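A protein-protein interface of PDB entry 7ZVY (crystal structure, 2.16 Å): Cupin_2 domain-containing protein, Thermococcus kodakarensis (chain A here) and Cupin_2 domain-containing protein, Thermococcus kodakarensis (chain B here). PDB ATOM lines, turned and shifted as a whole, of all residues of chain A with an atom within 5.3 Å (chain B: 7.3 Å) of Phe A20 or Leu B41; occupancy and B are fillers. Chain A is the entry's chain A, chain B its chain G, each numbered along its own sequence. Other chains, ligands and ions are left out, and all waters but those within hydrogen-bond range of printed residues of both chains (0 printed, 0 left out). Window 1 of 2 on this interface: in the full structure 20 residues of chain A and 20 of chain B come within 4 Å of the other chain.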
ATOM      1  N   MET A   1       6.305 -33.036 -18.235  1.00  0.00           N
ATOM      2  CA  MET A   1       6.666 -32.055 -17.171  1.00  0.00           C
ATOM      3  C   MET A   1       8.093 -31.537 -17.350  1.00  0.00           C
ATOM      4  O   MET A   1       8.242 -30.378 -17.787  1.00  0.00           O
ATOM      5  CB  MET A   1       6.507 -32.685 -15.786  1.00  0.00           C
ATOM      6  CG  MET A   1       5.069 -33.005 -15.410  1.00  0.00           C
ATOM      7  SD  MET A   1       4.917 -33.664 -13.740  1.00  0.00           S
ATOM      8  CE  MET A   1       5.503 -35.340 -13.983  1.00  0.00           C
ATOM      9  N   LYS A   2       9.102 -32.322 -16.957  1.00  0.00           N
ATOM     10  CA  LYS A   2      10.543 -32.009 -17.194  1.00  0.00           C
ATOM     11  C   LYS A   2      10.992 -32.349 -18.631  1.00  0.00           C
ATOM     12  O   LYS A   2      10.536 -33.376 -19.190  1.00  0.00           O
ATOM     13  CB  LYS A   2      11.418 -32.769 -16.202  1.00  0.00           C
ATOM     14  CG  LYS A   2      12.907 -32.729 -16.452  1.00  0.00           C
ATOM     15  CD  LYS A   2      13.611 -31.492 -16.052  1.00  0.00           C
ATOM     16  CE  LYS A   2      15.058 -31.845 -15.816  1.00  0.00           C
ATOM     17  NZ  LYS A   2      15.136 -32.793 -14.641  1.00  0.00           N
ATOM     18  N   ALA A   3      11.941 -31.544 -19.154  1.00  0.00           N
ATOM     19  CA  ALA A   3      12.454 -31.574 -20.550  1.00  0.00           C
ATOM     20  C   ALA A   3      13.678 -32.487 -20.690  1.00  0.00           C
ATOM     21  O   ALA A   3      14.755 -32.167 -20.087  1.00  0.00           O
ATOM     22  CB  ALA A   3      12.812 -30.178 -20.965  1.00  0.00           C
ATOM     23  N   PRO A  18      13.831 -30.635 -30.457  1.00  0.00           N
ATOM     24  CA  PRO A  18      12.514 -30.290 -29.945  1.00  0.00           C
ATOM     25  C   PRO A  18      12.246 -30.792 -28.510  1.00  0.00           C
ATOM     26  O   PRO A  18      12.948 -31.642 -27.981  1.00  0.00           O
ATOM     27  CB  PRO A  18      11.561 -30.947 -30.940  1.00  0.00           C
ATOM     28  CG  PRO A  18      12.408 -31.814 -31.856  1.00  0.00           C
ATOM     29  CD  PRO A  18      13.854 -31.484 -31.647  1.00  0.00           C
ATOM     30  N   LEU A  19      11.237 -30.192 -27.874  1.00  0.00           N
ATOM     31  CA  LEU A  19      10.942 -30.397 -26.451  1.00  0.00           C
ATOM     32  C   LEU A  19       9.453 -30.545 -26.330  1.00  0.00           C
ATOM     33  O   LEU A  19       8.747 -29.838 -27.073  1.00  0.00           O
ATOM     34  CB  LEU A  19      11.462 -29.212 -25.647  1.00  0.00           C
ATOM     35  CG  LEU A  19      12.945 -28.969 -25.802  1.00  0.00           C
ATOM     36  CD1 LEU A  19      13.269 -27.648 -25.165  1.00  0.00           C
ATOM     37  CD2 LEU A  19      13.739 -30.093 -25.151  1.00  0.00           C
ATOM     38  N   PHE A  20       9.023 -31.517 -25.514  1.00  0.00           N
ATOM     39  CA  PHE A  20       7.613 -31.704 -25.147  1.00  0.00           C
ATOM     40  C   PHE A  20       6.777 -31.887 -26.414  1.00  0.00           C
ATOM     41  O   PHE A  20       5.726 -31.253 -26.449  1.00  0.00           O
ATOM     42  CB  PHE A  20       7.023 -30.458 -24.499  1.00  0.00           C
ATOM     43  CG  PHE A  20       7.815 -29.945 -23.346  1.00  0.00           C
ATOM     44  CD1 PHE A  20       8.118 -30.790 -22.295  1.00  0.00           C
ATOM     45  CD2 PHE A  20       8.292 -28.638 -23.336  1.00  0.00           C
ATOM     46  CE1 PHE A  20       8.860 -30.333 -21.220  1.00  0.00           C
ATOM     47  CE2 PHE A  20       9.061 -28.212 -22.259  1.00  0.00           C
ATOM     48  CZ  PHE A  20       9.310 -29.055 -21.210  1.00  0.00           C
ATOM     49  N   GLU A  21       7.291 -32.572 -27.442  1.00  0.00           N
ATOM     50  CA  GLU A  21       6.588 -32.666 -28.748  1.00  0.00           C
ATOM     51  C   GLU A  21       5.276 -33.391 -28.463  1.00  0.00           C
ATOM     52  O   GLU A  21       5.321 -34.376 -27.685  1.00  0.00           O
ATOM     53  CB  GLU A  21       7.420 -33.407 -29.809  1.00  0.00           C
ATOM     54  CG  GLU A  21       8.923 -33.180 -29.703  1.00  0.00           C
ATOM     55  CD  GLU A  21       9.695 -34.178 -28.831  1.00  0.00           C
ATOM     56  OE1 GLU A  21       9.403 -34.260 -27.626  1.00  0.00           O
ATOM     57  OE2 GLU A  21      10.594 -34.880 -29.368  1.00  0.00           O
ATOM     58  N   GLY A  22       4.173 -32.907 -29.039  1.00  0.00           N
ATOM     59  CA  GLY A  22       2.828 -33.489 -28.912  1.00  0.00           C
ATOM     60  C   GLY A  22       2.145 -32.991 -27.650  1.00  0.00           C
ATOM     61  O   GLY A  22       0.900 -32.913 -27.615  1.00  0.00           O
ATOM     62  N   GLU A  23       2.930 -32.572 -26.654  1.00  0.00           N
ATOM     63  CA  GLU A  23       2.377 -32.164 -25.341  1.00  0.00           C
ATOM     64  C   GLU A  23       1.837 -30.754 -25.480  1.00  0.00           C
ATOM     65  O   GLU A  23       0.844 -30.438 -24.849  1.00  0.00           O
ATOM     66  CB  GLU A  23       3.445 -32.272 -24.255  1.00  0.00           C
ATOM     67  CG  GLU A  23       4.428 -33.399 -24.480  1.00  0.00           C
ATOM     68  CD  GLU A  23       3.852 -34.787 -24.577  1.00  0.00           C
ATOM     69  OE1 GLU A  23       2.663 -34.939 -24.218  1.00  0.00           O
ATOM     70  OE2 GLU A  23       4.627 -35.741 -24.921  1.00  0.00           O
ATOM     71  N   LEU A  24       2.412 -29.950 -26.371  1.00  0.00           N
ATOM     72  CA  LEU A  24       2.059 -28.519 -26.426  1.00  0.00           C
ATOM     73  C   LEU A  24       0.781 -28.298 -27.220  1.00  0.00           C
ATOM     74  O   LEU A  24       0.373 -29.116 -28.055  1.00  0.00           O
ATOM     75  CB  LEU A  24       3.254 -27.763 -26.983  1.00  0.00           C
ATOM     76  CG  LEU A  24       4.505 -27.911 -26.124  1.00  0.00           C
ATOM     77  CD1 LEU A  24       5.718 -27.305 -26.826  1.00  0.00           C
ATOM     78  CD2 LEU A  24       4.324 -27.260 -24.763  1.00  0.00           C
ATOM     79  N   ALA A  30       8.450 -25.728 -29.085  1.00  0.00           N
ATOM     80  CA  ALA A  30       9.576 -25.373 -28.218  1.00  0.00           C
ATOM     81  C   ALA A  30      10.726 -26.320 -28.461  1.00  0.00           C
ATOM     82  O   ALA A  30      10.513 -27.438 -28.933  1.00  0.00           O
ATOM     83  CB  ALA A  30       9.172 -25.349 -26.807  1.00  0.00           C
ATOM     84  N   PHE A  98      17.098 -21.538 -25.852  1.00  0.00           N
ATOM     85  CA  PHE A  98      15.723 -22.070 -25.688  1.00  0.00           C
ATOM     86  C   PHE A  98      14.844 -21.201 -26.535  1.00  0.00           C
ATOM     87  O   PHE A  98      14.971 -20.005 -26.392  1.00  0.00           O
ATOM     88  CB  PHE A  98      15.401 -22.042 -24.192  1.00  0.00           C
ATOM     89  CG  PHE A  98      14.004 -22.405 -23.818  1.00  0.00           C
ATOM     90  CD1 PHE A  98      13.464 -23.607 -24.228  1.00  0.00           C
ATOM     91  CD2 PHE A  98      13.234 -21.552 -23.056  1.00  0.00           C
ATOM     92  CE1 PHE A  98      12.168 -23.943 -23.917  1.00  0.00           C
ATOM     93  CE2 PHE A  98      11.957 -21.930 -22.674  1.00  0.00           C
ATOM     94  CZ  PHE A  98      11.441 -23.128 -23.072  1.00  0.00           C
ATOM     95  N   VAL A 100      10.830 -20.663 -28.051  1.00  0.00           N
ATOM     96  CA  VAL A 100       9.409 -21.061 -28.252  1.00  0.00           C
ATOM     97  C   VAL A 100       8.904 -20.344 -29.486  1.00  0.00           C
ATOM     98  O   VAL A 100       9.248 -19.197 -29.654  1.00  0.00           O
ATOM     99  CB  VAL A 100       8.600 -20.694 -27.012  1.00  0.00           C
ATOM    100  CG1 VAL A 100       7.186 -21.245 -27.108  1.00  0.00           C
ATOM    101  CG2 VAL A 100       9.356 -21.187 -25.756  1.00  0.00           C
ATOM    102  N   GLN B  20       7.305 -13.788 -19.326  1.00  0.00           N
ATOM    103  CA  GLN B  20       7.684 -12.960 -18.163  1.00  0.00           C
ATOM    104  C   GLN B  20       8.675 -13.736 -17.336  1.00  0.00           C
ATOM    105  O   GLN B  20       8.706 -14.958 -17.432  1.00  0.00           O
ATOM    106  CB  GLN B  20       6.440 -12.743 -17.318  1.00  0.00           C
ATOM    107  CG  GLN B  20       5.640 -14.015 -17.344  1.00  0.00           C
ATOM    108  CD  GLN B  20       4.621 -14.040 -16.252  1.00  0.00           C
ATOM    109  OE1 GLN B  20       5.008 -14.359 -15.138  1.00  0.00           O
ATOM    110  NE2 GLN B  20       3.372 -13.709 -16.569  1.00  0.00           N
ATOM    111  N   GLN B  38      -4.489 -22.594 -19.181  1.00  0.00           N
ATOM    112  CA  GLN B  38      -3.160 -22.135 -19.667  1.00  0.00           C
ATOM    113  C   GLN B  38      -2.045 -23.110 -19.304  1.00  0.00           C
ATOM    114  O   GLN B  38      -2.053 -23.746 -18.218  1.00  0.00           O
ATOM    115  CB  GLN B  38      -2.751 -20.729 -19.224  1.00  0.00           C
ATOM    116  CG  GLN B  38      -2.385 -20.605 -17.759  1.00  0.00           C
ATOM    117  CD  GLN B  38      -1.646 -19.324 -17.476  1.00  0.00           C
ATOM    118  OE1 GLN B  38      -0.413 -19.288 -17.470  1.00  0.00           O
ATOM    119  NE2 GLN B  38      -2.403 -18.257 -17.252  1.00  0.00           N
ATOM    120  N   TYR B  39      -1.070 -23.129 -20.211  1.00  0.00           N
ATOM    121  CA  TYR B  39       0.189 -23.888 -20.135  1.00  0.00           C
ATOM    122  C   TYR B  39       1.210 -22.943 -19.530  1.00  0.00           C
ATOM    123  O   TYR B  39       1.075 -21.707 -19.756  1.00  0.00           O
ATOM    124  CB  TYR B  39       0.593 -24.409 -21.508  1.00  0.00           C
ATOM    125  CG  TYR B  39      -0.335 -25.464 -22.037  1.00  0.00           C
ATOM    126  CD1 TYR B  39      -1.598 -25.099 -22.463  1.00  0.00           C
ATOM    127  CD2 TYR B  39       0.047 -26.794 -22.144  1.00  0.00           C
ATOM    128  CE1 TYR B  39      -2.484 -26.032 -22.957  1.00  0.00           C
ATOM    129  CE2 TYR B  39      -0.844 -27.747 -22.609  1.00  0.00           C
ATOM    130  CZ  TYR B  39      -2.095 -27.355 -23.038  1.00  0.00           C
ATOM    131  OH  TYR B  39      -2.980 -28.267 -23.532  1.00  0.00           O
ATOM    132  N   GLU B  40       2.105 -23.489 -18.707  1.00  0.00           N
ATOM    133  CA  GLU B  40       3.282 -22.774 -18.176  1.00  0.00           C
ATOM    134  C   GLU B  40       4.540 -23.455 -18.778  1.00  0.00           C
ATOM    135  O   GLU B  40       4.678 -24.674 -18.595  1.00  0.00           O
ATOM    136  CB  GLU B  40       3.206 -22.755 -16.631  1.00  0.00           C
ATOM    137  CG  GLU B  40       2.231 -21.745 -16.017  1.00  0.00           C
ATOM    138  CD  GLU B  40       2.410 -21.380 -14.541  1.00  0.00           C
ATOM    139  OE1 GLU B  40       2.121 -22.243 -13.603  1.00  0.00           O
ATOM    140  OE2 GLU B  40       2.766 -20.224 -14.283  1.00  0.00           O
ATOM    141  N   LEU B  41       5.394 -22.745 -19.549  1.00  0.00           N
ATOM    142  CA  LEU B  41       6.764 -23.253 -19.888  1.00  0.00           C
ATOM    143  C   LEU B  41       7.811 -22.596 -19.013  1.00  0.00           C
ATOM    144  O   LEU B  41       7.985 -21.432 -19.165  1.00  0.00           O
ATOM    145  CB  LEU B  41       7.110 -22.967 -21.346  1.00  0.00           C
ATOM    146  CG  LEU B  41       6.927 -24.166 -22.263  1.00  0.00           C
ATOM    147  CD1 LEU B  41       6.990 -23.738 -23.722  1.00  0.00           C
ATOM    148  CD2 LEU B  41       7.990 -25.167 -21.971  1.00  0.00           C
ATOM    149  N   PHE B  42       8.538 -23.351 -18.187  1.00  0.00           N
ATOM    150  CA  PHE B  42       9.596 -22.750 -17.334  1.00  0.00           C
ATOM    151  C   PHE B  42      10.960 -23.004 -17.941  1.00  0.00           C
ATOM    152  O   PHE B  42      11.278 -24.139 -18.292  1.00  0.00           O
ATOM    153  CB  PHE B  42       9.605 -23.360 -15.931  1.00  0.00           C
ATOM    154  CG  PHE B  42       8.301 -23.348 -15.168  1.00  0.00           C
ATOM    155  CD1 PHE B  42       7.349 -22.425 -15.474  1.00  0.00           C
ATOM    156  CD2 PHE B  42       8.068 -24.178 -14.075  1.00  0.00           C
ATOM    157  CE1 PHE B  42       6.147 -22.370 -14.781  1.00  0.00           C
ATOM    158  CE2 PHE B  42       6.863 -24.099 -13.364  1.00  0.00           C
ATOM    159  CZ  PHE B  42       5.940 -23.157 -13.701  1.00  0.00           C
ATOM    160  N   TYR B  43      11.813 -21.996 -17.917  1.00  0.00           N
ATOM    161  CA  TYR B  43      13.250 -22.286 -18.007  1.00  0.00           C
ATOM    162  C   TYR B  43      13.850 -21.725 -16.748  1.00  0.00           C
ATOM    163  O   TYR B  43      13.648 -20.553 -16.586  1.00  0.00           O
ATOM    164  CB  TYR B  43      13.862 -21.726 -19.305  1.00  0.00           C
ATOM    165  CG  TYR B  43      15.373 -21.822 -19.321  1.00  0.00           C
ATOM    166  CD1 TYR B  43      16.165 -20.834 -18.742  1.00  0.00           C
ATOM    167  CD2 TYR B  43      16.034 -22.864 -19.945  1.00  0.00           C
ATOM    168  CE1 TYR B  43      17.536 -20.967 -18.644  1.00  0.00           C
ATOM    169  CE2 TYR B  43      17.431 -22.959 -19.935  1.00  0.00           C
ATOM    170  CZ  TYR B  43      18.191 -22.006 -19.280  1.00  0.00           C
ATOM    171  OH  TYR B  43      19.584 -21.960 -19.272  1.00  0.00           O
ATOM    172  N   ILE B  65      14.285 -27.209 -18.020  1.00  0.00           N
ATOM    173  CA  ILE B  65      13.061 -26.685 -18.667  1.00  0.00           C
ATOM    174  C   ILE B  65      11.871 -27.524 -18.160  1.00  0.00           C
ATOM    175  O   ILE B  65      12.011 -28.748 -17.976  1.00  0.00           O
ATOM    176  CB  ILE B  65      13.256 -26.748 -20.165  1.00  0.00           C
ATOM    177  CG1 ILE B  65      14.301 -25.727 -20.594  1.00  0.00           C
ATOM    178  CG2 ILE B  65      11.965 -26.531 -20.927  1.00  0.00           C
ATOM    179  CD1 ILE B  65      14.832 -25.935 -21.979  1.00  0.00           C
ATOM    180  N   PHE B  66      10.759 -26.890 -17.814  1.00  0.00           N
ATOM    181  CA  PHE B  66       9.568 -27.649 -17.370  1.00  0.00           C
ATOM    182  C   PHE B  66       8.365 -27.182 -18.141  1.00  0.00           C
ATOM    183  O   PHE B  66       8.436 -26.067 -18.663  1.00  0.00           O
ATOM    184  CB  PHE B  66       9.289 -27.484 -15.881  1.00  0.00           C
ATOM    185  CG  PHE B  66      10.401 -28.012 -15.025  1.00  0.00           C
ATOM    186  CD1 PHE B  66      10.359 -29.312 -14.585  1.00  0.00           C
ATOM    187  CD2 PHE B  66      11.429 -27.199 -14.611  1.00  0.00           C
ATOM    188  CE1 PHE B  66      11.366 -29.817 -13.795  1.00  0.00           C
ATOM    189  CE2 PHE B  66      12.448 -27.702 -13.825  1.00  0.00           C
ATOM    190  CZ  PHE B  66      12.411 -29.014 -13.425  1.00  0.00           C
ATOM    191  N   LEU B  67       7.391 -28.077 -18.298  1.00  0.00           N
ATOM    192  CA  LEU B  67       6.052 -27.774 -18.839  1.00  0.00           C
ATOM    193  C   LEU B  67       5.038 -28.103 -17.744  1.00  0.00           C
ATOM    194  O   LEU B  67       5.129 -29.205 -17.145  1.00  0.00           O
ATOM    195  CB  LEU B  67       5.768 -28.600 -20.095  1.00  0.00           C
ATOM    196  CG  LEU B  67       4.345 -28.462 -20.567  1.00  0.00           C
ATOM    197  CD1 LEU B  67       4.194 -27.091 -21.201  1.00  0.00           C
ATOM    198  CD2 LEU B  67       3.952 -29.570 -21.540  1.00  0.00           C
ATOM    199  N   VAL B  68       4.162 -27.148 -17.456  1.00  0.00           N
ATOM    200  CA  VAL B  68       2.927 -27.331 -16.627  1.00  0.00           C
ATOM    201  C   VAL B  68       1.718 -27.256 -17.552  1.00  0.00           C
ATOM    202  O   VAL B  68       1.177 -26.158 -17.807  1.00  0.00           O
ATOM    203  CB  VAL B  68       2.817 -26.284 -15.495  1.00  0.00           C
ATOM    204  CG1 VAL B  68       1.506 -26.390 -14.736  1.00  0.00           C
ATOM    205  CG2 VAL B  68       3.965 -26.423 -14.505  1.00  0.00           C
ATOM    206  N   LYS B  69       1.181 -28.414 -17.954  1.00  0.00           N
ATOM    207  CA  LYS B  69      -0.107 -28.427 -18.682  1.00  0.00           C
ATOM    208  C   LYS B  69      -1.228 -28.050 -17.710  1.00  0.00           C
ATOM    209  O   LYS B  69      -1.030 -28.064 -16.498  1.00  0.00           O
ATOM    210  CB  LYS B  69      -0.352 -29.807 -19.275  1.00  0.00           C
ATOM    211  CG  LYS B  69       0.879 -30.476 -19.863  1.00  0.00           C
ATOM    212  CD  LYS B  69       0.508 -31.635 -20.771  1.00  0.00           C
ATOM    213  CE  LYS B  69      -0.779 -31.380 -21.553  1.00  0.00           C
ATOM    214  NZ  LYS B  69      -0.798 -32.033 -22.888  1.00  0.00           N
ATOM    215  N   LEU B  86      12.968 -17.804 -12.835  1.00  0.00           N
ATOM    216  CA  LEU B  86      12.672 -18.701 -13.986  1.00  0.00           C
ATOM    217  C   LEU B  86      12.108 -17.882 -15.134  1.00  0.00           C
ATOM    218  O   LEU B  86      11.590 -16.749 -14.894  1.00  0.00           O
ATOM    219  CB  LEU B  86      11.796 -19.904 -13.577  1.00  0.00           C
ATOM    220  CG  LEU B  86      10.536 -19.743 -12.711  1.00  0.00           C
ATOM    221  CD1 LEU B  86       9.894 -21.127 -12.493  1.00  0.00           C
ATOM    222  CD2 LEU B  86      10.843 -19.174 -11.327  1.00  0.00           C
ATOM    223  N   PHE B  87      12.262 -18.403 -16.353  1.00  0.00           N
ATOM    224  CA  PHE B  87      11.758 -17.711 -17.556  1.00  0.00           C
ATOM    225  C   PHE B  87      10.428 -18.391 -17.799  1.00  0.00           C
ATOM    226  O   PHE B  87      10.361 -19.628 -17.883  1.00  0.00           O
ATOM    227  CB  PHE B  87      12.763 -17.754 -18.730  1.00  0.00           C
ATOM    228  CG  PHE B  87      12.140 -17.249 -20.002  1.00  0.00           C
ATOM    229  CD1 PHE B  87      11.705 -15.942 -20.101  1.00  0.00           C
ATOM    230  CD2 PHE B  87      12.008 -18.083 -21.110  1.00  0.00           C
ATOM    231  CE1 PHE B  87      11.121 -15.482 -21.272  1.00  0.00           C
ATOM    232  CE2 PHE B  87      11.393 -17.622 -22.259  1.00  0.00           C
ATOM    233  CZ  PHE B  87      10.933 -16.336 -22.326  1.00  0.00           C
ATOM    234  N   VAL B  88       9.361 -17.626 -17.896  1.00  0.00           N
ATOM    235  CA  VAL B  88       8.061 -18.307 -18.042  1.00  0.00           C
ATOM    236  C   VAL B  88       7.436 -17.933 -19.367  1.00  0.00           C
ATOM    237  O   VAL B  88       7.459 -16.770 -19.795  1.00  0.00           O
ATOM    238  CB  VAL B  88       7.141 -17.989 -16.864  1.00  0.00           C
ATOM    239  CG1 VAL B  88       5.747 -18.500 -17.136  1.00  0.00           C
ATOM    240  CG2 VAL B  88       7.744 -18.545 -15.582  1.00  0.00           C
ATOM    241  N   VAL B  89       6.862 -18.936 -20.003  1.00  0.00           N
ATOM    242  CA  VAL B  89       5.987 -18.598 -21.152  1.00  0.00           C
ATOM    243  C   VAL B  89       4.617 -19.245 -20.906  1.00  0.00           C
ATOM    244  O   VAL B  89       4.493 -20.349 -20.362  1.00  0.00           O
ATOM    245  CB  VAL B  89       6.657 -18.927 -22.497  1.00  0.00           C
ATOM    246  CG1 VAL B  89       5.869 -18.296 -23.630  1.00  0.00           C
ATOM    247  CG2 VAL B  89       8.092 -18.444 -22.500  1.00  0.00           C
ATOM    248  N   LYS B  90       3.565 -18.515 -21.222  1.00  0.00           N
ATOM    249  CA  LYS B  90       2.240 -19.080 -20.939  1.00  0.00           C
ATOM    250  C   LYS B  90       1.532 -19.270 -22.266  1.00  0.00           C
ATOM    251  O   LYS B  90       1.462 -18.335 -23.075  1.00  0.00           O
ATOM    252  CB  LYS B  90       1.494 -18.221 -19.912  1.00  0.00           C
ATOM    253  CG  LYS B  90       2.287 -18.048 -18.622  1.00  0.00           C
ATOM    254  CD  LYS B  90       1.583 -17.165 -17.580  1.00  0.00           C
ATOM    255  CE  LYS B  90       2.361 -17.108 -16.276  1.00  0.00           C
ATOM    256  NZ  LYS B  90       2.305 -18.384 -15.507  1.00  0.00           N
ATOM    257  N   LEU B  91       1.031 -20.477 -22.479  1.00  0.00           N
ATOM    258  CA  LEU B  91       0.358 -20.796 -23.744  1.00  0.00           C
ATOM    259  C   LEU B  91      -1.111 -21.064 -23.475  1.00  0.00           C
ATOM    260  O   LEU B  91      -1.486 -21.444 -22.312  1.00  0.00           O
ATOM    261  CB  LEU B  91       1.028 -22.002 -24.392  1.00  0.00           C
ATOM    262  CG  LEU B  91       2.530 -21.877 -24.633  1.00  0.00           C
ATOM    263  CD1 LEU B  91       3.015 -23.151 -25.284  1.00  0.00           C
ATOM    264  CD2 LEU B  91       2.866 -20.672 -25.520  1.00  0.00           C
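The backbone carbonyl oxygen of Met A1 lies within hydrogen-bond range of the backbone NH of Leu B67, 2.5 Å away.
N of Ala A3 is in hydrogen-bond range of O of Ile B65 (3.0 Å).
O of Glu A23 lies within hydrogen-bond range of NZ of Lys B69 (3.0 Å).
Of the 13 printed residues of chain A, 8 touch a printed residue of chain B.
Along chain A the printed residues that touch a printed residue of chain B span positions 1 to 98.
Of the 18 printed residues of chain B, 7 touch a printed residue of chain A.
Hydrophobic or aromatic side chains of chain B within 4 Å of the printed part of chain A: Tyr B39, Leu B41, Tyr B43, Ile B65, Phe B66 and Leu B67.
Among the printed residues, 16 pairs touch across the chains.
Among the printed residues, no Asp or Glu carboxylate lies within 4 Å of a Lys or Arg side-chain nitrogen of the other chain.
N of Leu A19 is in hydrogen-bond range of O of Ala A30 (3.0 Å).
The backbone NH of Tyr B39 lies within hydrogen-bond range of the backbone carbonyl oxygen of Leu B91.
The backbone NH (N) of Leu B41 sits at hydrogen-bond distance from the backbone carbonyl oxygen (O) of Val B89.
The backbone NH (N) of Phe B42 lies within hydrogen-bond range of the backbone carbonyl oxygen (O) of Phe B66.
The backbone carbonyl oxygen of Tyr B43 is in hydrogen-bond range of the backbone NH of Phe B87 (2.6 Å).
CA of Phe B66 touches O of Met A1 (3.1 Å).
CA of Lys A2 touches O of Ile B65 (3.7 Å).
Lys A2 touches Phe B66 (CD to CE1, 3.6 Å).
CE2 of Phe A20 touches CD2 of Leu B41, 3.2 Å away.
Ile B65 touches Phe A20.
Phe B66 touches Phe A20.
Tyr B39 touches Glu A23.
Leu B67 touches Glu A23 (CD2 to CB, 3.9 Å).
CD1 of Leu B67 touches CD2 of Leu A24, at 3.6 Å.
Tyr B43 touches Phe A98 (CB to CD2, 3.8 Å).
Printed residues of chain B within 4 Å of Met A1: Phe B66 and Leu B67.
Phe A20 touches just these residues of chain B: Leu B41, Ile B65, Phe B66 and Leu B67.
Printed residues of chain A within 4 Å of Leu B41: Phe A20.
Of the printed residues of chain A, Lys B69 touches Glu A23 (3.0 Å).
The nearest residue of chain B that does not touch Phe A20 is Phe B42 (6.0 Å).
The nearest printed residue of chain B that does not touch Glu A23 is Leu B91 (7.6 Å).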
